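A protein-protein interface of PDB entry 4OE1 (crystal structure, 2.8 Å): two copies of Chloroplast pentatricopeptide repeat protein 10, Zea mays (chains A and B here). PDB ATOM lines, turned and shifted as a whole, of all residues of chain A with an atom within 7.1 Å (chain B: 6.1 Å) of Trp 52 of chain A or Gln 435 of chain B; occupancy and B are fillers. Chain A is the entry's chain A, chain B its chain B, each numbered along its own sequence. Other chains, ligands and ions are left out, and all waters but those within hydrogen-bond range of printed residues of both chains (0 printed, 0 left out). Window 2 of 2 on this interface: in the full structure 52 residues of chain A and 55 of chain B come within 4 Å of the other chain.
No position is printed for both chains. Of the 6 pairs that touch across the chains among the printed residues, none has its exchanged pair printed and touching as well.
Among the printed residues, merely in contact across the chains: Trp 52 of chain A with Gln 435 of chain B, Glu 53 of chain A with Gln 435 of chain B, Glu 53 of chain A with Gly 436 of chain B and Asp 87 of chain A with Gly 401 of chain B.
Of chain B, only Gln 435 comes within 4 Å of Trp 52 of chain A. Of the printed residues of chain B, Gln 85 of chain A touches Gln 435. Of the printed residues of chain A, Gly 401 of chain B touches Asp 87. Gln 435 of chain B touches just these residues of chain A: Trp 52, Glu 53 and Gln 85. The nearest residue of chain A that does not touch Gln 435 of chain B is Ala 88 of chain A (6.0 Å). The nearest printed residue of chain B that does not touch Asp 87 of chain A is Gln 435 of chain B (6.2 Å).
OD2 of Asp 87 of chain A is in hydrogen-bond range of N of Arg 403 of chain B, 3.5 Å away. The side-chain amide oxygen of Gln 85 of chain A is in hydrogen-bond range of the side-chain amide nitrogen of Gln 435 of chain B, at 3.0 Å.
The side-chain carboxylate (OD2) of Asp 437 of chain B is in salt-bridge range of the guanidinium group (NH2) of Arg 403 of chain B. NH1 of Arg 403 of chain B lies within hydrogen-bond range of OE1 of Gln 435 of chain B, 3.2 Å away. The backbone carbonyl oxygen (O) of Leu 80 of chain A lies within hydrogen-bond range of the backbone NH (N) of Gln 85 of chain A (2.4 Å).
Of the 20 printed residues of chain A, 4 touch a printed residue of chain B. Printed residues of chain A that touch a printed residue of chain B: Trp 52, Glu 53, Gln 85 and Asp 87. Along chain B the printed residues that touch a printed residue of chain A span positions 401 to 436. Among the printed residues, no Asp or Glu carboxylate lies within 4 Å of a Lys or Arg side-chain nitrogen of the other chain.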
ATOM      1  N   LEU A  43       4.865  23.139  18.237  1.00  0.00           N
ATOM      2  CA  LEU A  43       3.488  22.668  18.152  1.00  0.00           C
ATOM      3  C   LEU A  43       2.986  22.692  16.713  1.00  0.00           C
ATOM      4  O   LEU A  43       2.407  21.718  16.232  1.00  0.00           O
ATOM      5  CB  LEU A  43       2.580  23.512  19.044  1.00  0.00           C
ATOM      6  CG  LEU A  43       2.928  23.535  20.533  1.00  0.00           C
ATOM      7  CD1 LEU A  43       1.698  23.875  21.360  1.00  0.00           C
ATOM      8  CD2 LEU A  43       3.520  22.205  20.968  1.00  0.00           C
ATOM      9  N   LEU A  46       4.609  19.933  14.818  1.00  0.00           N
ATOM     10  CA  LEU A  46       4.175  18.595  15.150  1.00  0.00           C
ATOM     11  C   LEU A  46       2.826  18.286  14.525  1.00  0.00           C
ATOM     12  O   LEU A  46       2.530  17.141  14.233  1.00  0.00           O
ATOM     13  CB  LEU A  46       4.118  18.416  16.656  1.00  0.00           C
ATOM     14  CG  LEU A  46       5.470  18.466  17.365  1.00  0.00           C
ATOM     15  CD1 LEU A  46       5.300  18.739  18.837  1.00  0.00           C
ATOM     16  CD2 LEU A  46       6.193  17.169  17.181  1.00  0.00           C
ATOM     17  N   GLU A  47       2.014  19.321  14.321  1.00  0.00           N
ATOM     18  CA  GLU A  47       0.697  19.156  13.724  1.00  0.00           C
ATOM     19  C   GLU A  47       0.786  19.058  12.206  1.00  0.00           C
ATOM     20  O   GLU A  47      -0.086  18.479  11.557  1.00  0.00           O
ATOM     21  CB  GLU A  47      -0.222  20.312  14.123  1.00  0.00           C
ATOM     22  CG  GLU A  47      -0.590  20.332  15.599  1.00  0.00           C
ATOM     23  CD  GLU A  47      -1.470  21.512  15.962  1.00  0.00           C
ATOM     24  OE1 GLU A  47      -2.025  22.148  15.043  1.00  0.00           O
ATOM     25  OE2 GLU A  47      -1.608  21.801  17.171  1.00  0.00           O
ATOM     26  N   LEU A  48       1.847  19.632  11.642  1.00  0.00           N
ATOM     27  CA  LEU A  48       2.052  19.610  10.201  1.00  0.00           C
ATOM     28  C   LEU A  48       2.355  18.202   9.707  1.00  0.00           C
ATOM     29  O   LEU A  48       2.403  17.954   8.501  1.00  0.00           O
ATOM     30  CB  LEU A  48       3.187  20.560   9.807  1.00  0.00           C
ATOM     31  CG  LEU A  48       3.517  20.645   8.316  1.00  0.00           C
ATOM     32  CD1 LEU A  48       2.634  21.679   7.628  1.00  0.00           C
ATOM     33  CD2 LEU A  48       4.987  20.965   8.107  1.00  0.00           C
ATOM     34  N   SER A  49       2.557  17.281  10.643  1.00  0.00           N
ATOM     35  CA  SER A  49       2.854  15.895  10.308  1.00  0.00           C
ATOM     36  C   SER A  49       1.808  14.949  10.893  1.00  0.00           C
ATOM     37  O   SER A  49       1.963  13.728  10.839  1.00  0.00           O
ATOM     38  CB  SER A  49       4.249  15.510  10.803  1.00  0.00           C
ATOM     39  OG  SER A  49       4.319  15.564  12.217  1.00  0.00           O
ATOM     40  N   GLY A  50       0.746  15.525  11.450  1.00  0.00           N
ATOM     41  CA  GLY A  50      -0.317  14.735  12.045  1.00  0.00           C
ATOM     42  C   GLY A  50       0.096  14.082  13.345  1.00  0.00           C
ATOM     43  O   GLY A  50      -0.444  13.049  13.734  1.00  0.00           O
ATOM     44  N   HIS A  51       1.085  14.664  14.011  1.00  0.00           N
ATOM     45  CA  HIS A  51       1.555  14.139  15.283  1.00  0.00           C
ATOM     46  C   HIS A  51       0.949  14.961  16.406  1.00  0.00           C
ATOM     47  O   HIS A  51       1.666  15.537  17.225  1.00  0.00           O
ATOM     48  CB  HIS A  51       3.082  14.190  15.357  1.00  0.00           C
ATOM     49  CG  HIS A  51       3.762  13.080  14.621  1.00  0.00           C
ATOM     50  ND1 HIS A  51       4.446  13.274  13.442  1.00  0.00           N
ATOM     51  CD2 HIS A  51       3.860  11.755  14.897  1.00  0.00           C
ATOM     52  CE1 HIS A  51       4.939  12.122  13.023  1.00  0.00           C
ATOM     53  NE2 HIS A  51       4.597  11.184  13.888  1.00  0.00           N
ATOM     54  N   TRP A  52      -0.375  15.026  16.443  1.00  0.00           N
ATOM     55  CA  TRP A  52      -1.041  15.902  17.387  1.00  0.00           C
ATOM     56  C   TRP A  52      -1.041  15.379  18.798  1.00  0.00           C
ATOM     57  O   TRP A  52      -1.168  16.146  19.742  1.00  0.00           O
ATOM     58  CB  TRP A  52      -2.468  16.199  16.939  1.00  0.00           C
ATOM     59  CG  TRP A  52      -3.337  15.001  16.809  1.00  0.00           C
ATOM     60  CD1 TRP A  52      -3.656  14.342  15.667  1.00  0.00           C
ATOM     61  CD2 TRP A  52      -4.015  14.325  17.862  1.00  0.00           C
ATOM     62  NE1 TRP A  52      -4.487  13.297  15.939  1.00  0.00           N
ATOM     63  CE2 TRP A  52      -4.719  13.266  17.289  1.00  0.00           C
ATOM     64  CE3 TRP A  52      -4.088  14.514  19.241  1.00  0.00           C
ATOM     65  CZ2 TRP A  52      -5.484  12.406  18.039  1.00  0.00           C
ATOM     66  CZ3 TRP A  52      -4.847  13.658  19.980  1.00  0.00           C
ATOM     67  CH2 TRP A  52      -5.534  12.617  19.384  1.00  0.00           C
ATOM     68  N   GLU A  53      -0.897  14.072  18.952  1.00  0.00           N
ATOM     69  CA  GLU A  53      -0.866  13.494  20.288  1.00  0.00           C
ATOM     70  C   GLU A  53       0.416  13.900  20.973  1.00  0.00           C
ATOM     71  O   GLU A  53       0.507  13.913  22.193  1.00  0.00           O
ATOM     72  CB  GLU A  53      -0.945  11.972  20.247  1.00  0.00           C
ATOM     73  CG  GLU A  53      -2.112  11.420  19.490  1.00  0.00           C
ATOM     74  CD  GLU A  53      -1.722  10.992  18.114  1.00  0.00           C
ATOM     75  OE1 GLU A  53      -1.174  11.824  17.368  1.00  0.00           O
ATOM     76  OE2 GLU A  53      -1.955   9.820  17.772  1.00  0.00           O
ATOM     77  N   TRP A  54       1.403  14.246  20.160  1.00  0.00           N
ATOM     78  CA  TRP A  54       2.712  14.635  20.627  1.00  0.00           C
ATOM     79  C   TRP A  54       2.763  16.115  20.966  1.00  0.00           C
ATOM     80  O   TRP A  54       3.477  16.524  21.869  1.00  0.00           O
ATOM     81  CB  TRP A  54       3.761  14.290  19.573  1.00  0.00           C
ATOM     82  CG  TRP A  54       4.094  12.842  19.532  1.00  0.00           C
ATOM     83  CD1 TRP A  54       4.982  12.195  20.322  1.00  0.00           C
ATOM     84  CD2 TRP A  54       3.544  11.853  18.661  1.00  0.00           C
ATOM     85  NE1 TRP A  54       5.024  10.869  20.003  1.00  0.00           N
ATOM     86  CE2 TRP A  54       4.147  10.634  18.983  1.00  0.00           C
ATOM     87  CE3 TRP A  54       2.597  11.884  17.645  1.00  0.00           C
ATOM     88  CZ2 TRP A  54       3.839   9.463  18.325  1.00  0.00           C
ATOM     89  CZ3 TRP A  54       2.294  10.720  16.993  1.00  0.00           C
ATOM     90  CH2 TRP A  54       2.912   9.528  17.330  1.00  0.00           C
ATOM     91  N   ALA A  55       1.989  16.911  20.252  1.00  0.00           N
ATOM     92  CA  ALA A  55       1.921  18.330  20.512  1.00  0.00           C
ATOM     93  C   ALA A  55       1.198  18.586  21.809  1.00  0.00           C
ATOM     94  O   ALA A  55       1.337  19.634  22.414  1.00  0.00           O
ATOM     95  CB  ALA A  55       1.229  19.020  19.391  1.00  0.00           C
ATOM     96  N   LEU A  56       0.422  17.611  22.242  1.00  0.00           N
ATOM     97  CA  LEU A  56      -0.293  17.720  23.491  1.00  0.00           C
ATOM     98  C   LEU A  56       0.637  17.401  24.637  1.00  0.00           C
ATOM     99  O   LEU A  56       0.649  18.083  25.643  1.00  0.00           O
ATOM    100  CB  LEU A  56      -1.451  16.739  23.495  1.00  0.00           C
ATOM    101  CG  LEU A  56      -2.783  17.175  24.084  1.00  0.00           C
ATOM    102  CD1 LEU A  56      -3.646  15.974  24.256  1.00  0.00           C
ATOM    103  CD2 LEU A  56      -2.593  17.837  25.402  1.00  0.00           C
ATOM    104  N   ALA A  57       1.416  16.350  24.471  1.00  0.00           N
ATOM    105  CA  ALA A  57       2.292  15.898  25.526  1.00  0.00           C
ATOM    106  C   ALA A  57       3.329  16.942  25.859  1.00  0.00           C
ATOM    107  O   ALA A  57       3.750  17.073  26.999  1.00  0.00           O
ATOM    108  CB  ALA A  57       2.961  14.631  25.113  1.00  0.00           C
ATOM    109  N   VAL A  76      -2.944  24.159  20.000  1.00  0.00           N
ATOM    110  CA  VAL A  76      -3.174  22.742  20.128  1.00  0.00           C
ATOM    111  C   VAL A  76      -4.661  22.464  20.056  1.00  0.00           C
ATOM    112  O   VAL A  76      -5.097  21.478  19.487  1.00  0.00           O
ATOM    113  CB  VAL A  76      -2.577  22.225  21.422  1.00  0.00           C
ATOM    114  CG1 VAL A  76      -3.058  20.852  21.711  1.00  0.00           C
ATOM    115  CG2 VAL A  76      -1.091  22.220  21.320  1.00  0.00           C
ATOM    116  N   ALA A  79      -6.327  22.248  16.513  1.00  0.00           N
ATOM    117  CA  ALA A  79      -6.096  20.955  15.913  1.00  0.00           C
ATOM    118  C   ALA A  79      -7.024  19.911  16.487  1.00  0.00           C
ATOM    119  O   ALA A  79      -7.699  19.208  15.758  1.00  0.00           O
ATOM    120  CB  ALA A  79      -4.681  20.556  16.134  1.00  0.00           C
ATOM    121  N   LEU A  80      -7.041  19.818  17.808  1.00  0.00           N
ATOM    122  CA  LEU A  80      -7.875  18.862  18.491  1.00  0.00           C
ATOM    123  C   LEU A  80      -9.303  18.993  18.039  1.00  0.00           C
ATOM    124  O   LEU A  80      -9.972  18.009  17.763  1.00  0.00           O
ATOM    125  CB  LEU A  80      -7.807  19.080  19.989  1.00  0.00           C
ATOM    126  CG  LEU A  80      -6.513  18.641  20.642  1.00  0.00           C
ATOM    127  CD1 LEU A  80      -6.612  18.721  22.134  1.00  0.00           C
ATOM    128  CD2 LEU A  80      -6.196  17.257  20.225  1.00  0.00           C
ATOM    129  N   GLU A  83      -9.336  17.953  14.664  1.00  0.00           N
ATOM    130  CA  GLU A  83      -9.098  16.543  14.565  1.00  0.00           C
ATOM    131  C   GLU A  83     -10.128  15.829  15.381  1.00  0.00           C
ATOM    132  O   GLU A  83     -10.059  14.641  15.555  1.00  0.00           O
ATOM    133  CB  GLU A  83      -7.702  16.239  15.071  1.00  0.00           C
ATOM    134  CG  GLU A  83      -7.027  15.081  14.456  1.00  0.00           C
ATOM    135  CD  GLU A  83      -6.779  15.263  13.004  1.00  0.00           C
ATOM    136  OE1 GLU A  83      -6.912  14.284  12.261  1.00  0.00           O
ATOM    137  OE2 GLU A  83      -6.434  16.369  12.588  1.00  0.00           O
ATOM    138  N   GLN A  85     -11.045  15.973  18.601  1.00  0.00           N
ATOM    139  CA  GLN A  85     -10.647  15.386  19.859  1.00  0.00           C
ATOM    140  C   GLN A  85     -11.167  16.115  21.060  1.00  0.00           C
ATOM    141  O   GLN A  85     -10.422  16.714  21.803  1.00  0.00           O
ATOM    142  CB  GLN A  85      -9.143  15.286  19.921  1.00  0.00           C
ATOM    143  CG  GLN A  85      -8.608  14.268  18.988  1.00  0.00           C
ATOM    144  CD  GLN A  85      -9.135  12.917  19.316  1.00  0.00           C
ATOM    145  OE1 GLN A  85      -9.338  12.594  20.476  1.00  0.00           O
ATOM    146  NE2 GLN A  85      -9.379  12.117  18.303  1.00  0.00           N
ATOM    147  N   ASP A  87     -12.473  15.173  23.973  1.00  0.00           N
ATOM    148  CA  ASP A  87     -12.189  14.770  25.339  1.00  0.00           C
ATOM    149  C   ASP A  87     -10.886  15.365  25.771  1.00  0.00           C
ATOM    150  O   ASP A  87     -10.678  15.659  26.935  1.00  0.00           O
ATOM    151  CB  ASP A  87     -12.111  13.254  25.459  1.00  0.00           C
ATOM    152  CG  ASP A  87     -11.668  12.802  26.833  1.00  0.00           C
ATOM    153  OD1 ASP A  87     -12.477  12.860  27.770  1.00  0.00           O
ATOM    154  OD2 ASP A  87     -10.514  12.381  26.973  1.00  0.00           O
ATOM    155  N   ALA A  88     -10.005  15.548  24.812  1.00  0.00           N
ATOM    156  CA  ALA A  88      -8.667  15.981  25.101  1.00  0.00           C
ATOM    157  C   ALA A  88      -8.667  17.440  25.466  1.00  0.00           C
ATOM    158  O   ALA A  88      -7.830  17.898  26.221  1.00  0.00           O
ATOM    159  CB  ALA A  88      -7.810  15.741  23.910  1.00  0.00           C
ATOM    160  N   GLY B 401     -16.107   8.112  24.175  1.00  0.00           N
ATOM    161  CA  GLY B 401     -14.814   8.476  23.642  1.00  0.00           C
ATOM    162  C   GLY B 401     -14.006   9.252  24.653  1.00  0.00           C
ATOM    163  O   GLY B 401     -13.067   9.944  24.308  1.00  0.00           O
ATOM    164  N   ARG B 403     -11.391   9.027  26.704  1.00  0.00           N
ATOM    165  CA  ARG B 403     -10.177   8.297  27.039  1.00  0.00           C
ATOM    166  C   ARG B 403      -9.744   8.613  28.440  1.00  0.00           C
ATOM    167  O   ARG B 403      -9.196   7.792  29.148  1.00  0.00           O
ATOM    168  CB  ARG B 403      -9.051   8.695  26.093  1.00  0.00           C
ATOM    169  CG  ARG B 403      -7.710   8.116  26.454  1.00  0.00           C
ATOM    170  CD  ARG B 403      -6.572   9.019  26.037  1.00  0.00           C
ATOM    171  NE  ARG B 403      -5.287   8.349  26.137  1.00  0.00           N
ATOM    172  CZ  ARG B 403      -4.601   7.902  25.097  1.00  0.00           C
ATOM    173  NH1 ARG B 403      -5.072   8.061  23.878  1.00  0.00           N
ATOM    174  NH2 ARG B 403      -3.443   7.306  25.274  1.00  0.00           N
ATOM    175  N   ASN B 430     -10.225  -0.084  22.502  1.00  0.00           N
ATOM    176  CA  ASN B 430     -11.248   0.415  21.614  1.00  0.00           C
ATOM    177  C   ASN B 430     -11.081   1.884  21.472  1.00  0.00           C
ATOM    178  O   ASN B 430     -11.130   2.436  20.399  1.00  0.00           O
ATOM    179  CB  ASN B 430     -12.623   0.125  22.186  1.00  0.00           C
ATOM    180  CG  ASN B 430     -13.726   0.734  21.388  1.00  0.00           C
ATOM    181  OD1 ASN B 430     -13.701   0.732  20.170  1.00  0.00           O
ATOM    182  ND2 ASN B 430     -14.712   1.271  22.071  1.00  0.00           N
ATOM    183  N   VAL B 431     -10.875   2.509  22.598  1.00  0.00           N
ATOM    184  CA  VAL B 431     -10.700   3.931  22.687  1.00  0.00           C
ATOM    185  C   VAL B 431      -9.612   4.376  21.753  1.00  0.00           C
ATOM    186  O   VAL B 431      -9.869   5.035  20.764  1.00  0.00           O
ATOM    187  CB  VAL B 431     -10.292   4.311  24.084  1.00  0.00           C
ATOM    188  CG1 VAL B 431     -10.129   5.785  24.169  1.00  0.00           C
ATOM    189  CG2 VAL B 431     -11.322   3.859  25.050  1.00  0.00           C
ATOM    190  N   LEU B 432      -8.394   3.970  22.070  1.00  0.00           N
ATOM    191  CA  LEU B 432      -7.209   4.393  21.348  1.00  0.00           C
ATOM    192  C   LEU B 432      -7.401   4.215  19.874  1.00  0.00           C
ATOM    193  O   LEU B 432      -6.874   4.965  19.070  1.00  0.00           O
ATOM    194  CB  LEU B 432      -6.022   3.568  21.812  1.00  0.00           C
ATOM    195  CG  LEU B 432      -5.980   3.426  23.329  1.00  0.00           C
ATOM    196  CD1 LEU B 432      -4.973   2.405  23.741  1.00  0.00           C
ATOM    197  CD2 LEU B 432      -5.657   4.738  23.947  1.00  0.00           C
ATOM    198  N   SER B 433      -8.191   3.220  19.530  1.00  0.00           N
ATOM    199  CA  SER B 433      -8.442   2.897  18.156  1.00  0.00           C
ATOM    200  C   SER B 433      -9.101   4.051  17.452  1.00  0.00           C
ATOM    201  O   SER B 433      -8.878   4.279  16.269  1.00  0.00           O
ATOM    202  CB  SER B 433      -9.322   1.671  18.071  1.00  0.00           C
ATOM    203  OG  SER B 433      -9.266   1.146  16.768  1.00  0.00           O
ATOM    204  N   ARG B 434      -9.917   4.777  18.188  1.00  0.00           N
ATOM    205  CA  ARG B 434     -10.653   5.861  17.588  1.00  0.00           C
ATOM    206  C   ARG B 434      -9.696   6.949  17.207  1.00  0.00           C
ATOM    207  O   ARG B 434      -9.857   7.588  16.182  1.00  0.00           O
ATOM    208  CB  ARG B 434     -11.675   6.407  18.567  1.00  0.00           C
ATOM    209  N   GLN B 435      -8.703   7.133  18.058  1.00  0.00           N
ATOM    210  CA  GLN B 435      -7.770   8.199  17.885  1.00  0.00           C
ATOM    211  C   GLN B 435      -6.517   7.790  17.214  1.00  0.00           C
ATOM    212  O   GLN B 435      -5.644   8.585  17.084  1.00  0.00           O
ATOM    213  CB  GLN B 435      -7.426   8.850  19.199  1.00  0.00           C
ATOM    214  CG  GLN B 435      -7.744   8.110  20.424  1.00  0.00           C
ATOM    215  CD  GLN B 435      -7.803   9.019  21.616  1.00  0.00           C
ATOM    216  OE1 GLN B 435      -8.027   8.604  22.731  1.00  0.00           O
ATOM    217  NE2 GLN B 435      -7.608  10.266  21.388  1.00  0.00           N
ATOM    218  N   GLY B 436      -6.423   6.551  16.793  1.00  0.00           N
ATOM    219  CA  GLY B 436      -5.268   6.063  16.079  1.00  0.00           C
ATOM    220  C   GLY B 436      -4.009   6.134  16.901  1.00  0.00           C
ATOM    221  O   GLY B 436      -2.909   6.266  16.377  1.00  0.00           O
ATOM    222  N   ASP B 437      -4.168   6.046  18.211  1.00  0.00           N
ATOM    223  CA  ASP B 437      -3.027   6.048  19.101  1.00  0.00           C
ATOM    224  C   ASP B 437      -2.525   4.632  19.287  1.00  0.00           C
ATOM    225  O   ASP B 437      -3.027   3.886  20.111  1.00  0.00           O
ATOM    226  CB  ASP B 437      -3.397   6.661  20.443  1.00  0.00           C
ATOM    227  CG  ASP B 437      -2.236   6.720  21.375  1.00  0.00           C
ATOM    228  OD1 ASP B 437      -1.091   6.636  20.896  1.00  0.00           O
ATOM    229  OD2 ASP B 437      -2.455   6.845  22.589  1.00  0.00           O
ATOM    230  N   CYS B 466      -5.817   1.157  14.990  1.00  0.00           N
ATOM    231  CA  CYS B 466      -4.994   2.197  15.580  1.00  0.00           C
ATOM    232  C   CYS B 466      -3.910   2.549  14.600  1.00  0.00           C
ATOM    233  O   CYS B 466      -3.622   3.713  14.377  1.00  0.00           O
ATOM    234  CB  CYS B 466      -4.343   1.722  16.860  1.00  0.00           C
ATOM    235  SG  CYS B 466      -5.408   1.473  18.247  1.00  0.00           S
ATOM    236  N   LYS B 469      -5.010   4.588  11.416  1.00  0.00           N
ATOM    237  CA  LYS B 469      -5.220   5.981  11.739  1.00  0.00           C
ATOM    238  C   LYS B 469      -3.950   6.558  12.292  1.00  0.00           C
ATOM    239  O   LYS B 469      -3.920   7.693  12.739  1.00  0.00           O
ATOM    240  CB  LYS B 469      -6.316   6.136  12.773  1.00  0.00           C
ATOM    241  CG  LYS B 469      -7.697   6.123  12.205  1.00  0.00           C
ATOM    242  CD  LYS B 469      -8.646   6.773  13.175  1.00  0.00           C
ATOM    243  CE  LYS B 469      -8.185   8.180  13.523  1.00  0.00           C
ATOM    244  NZ  LYS B 469      -8.017   9.059  12.333  1.00  0.00           N
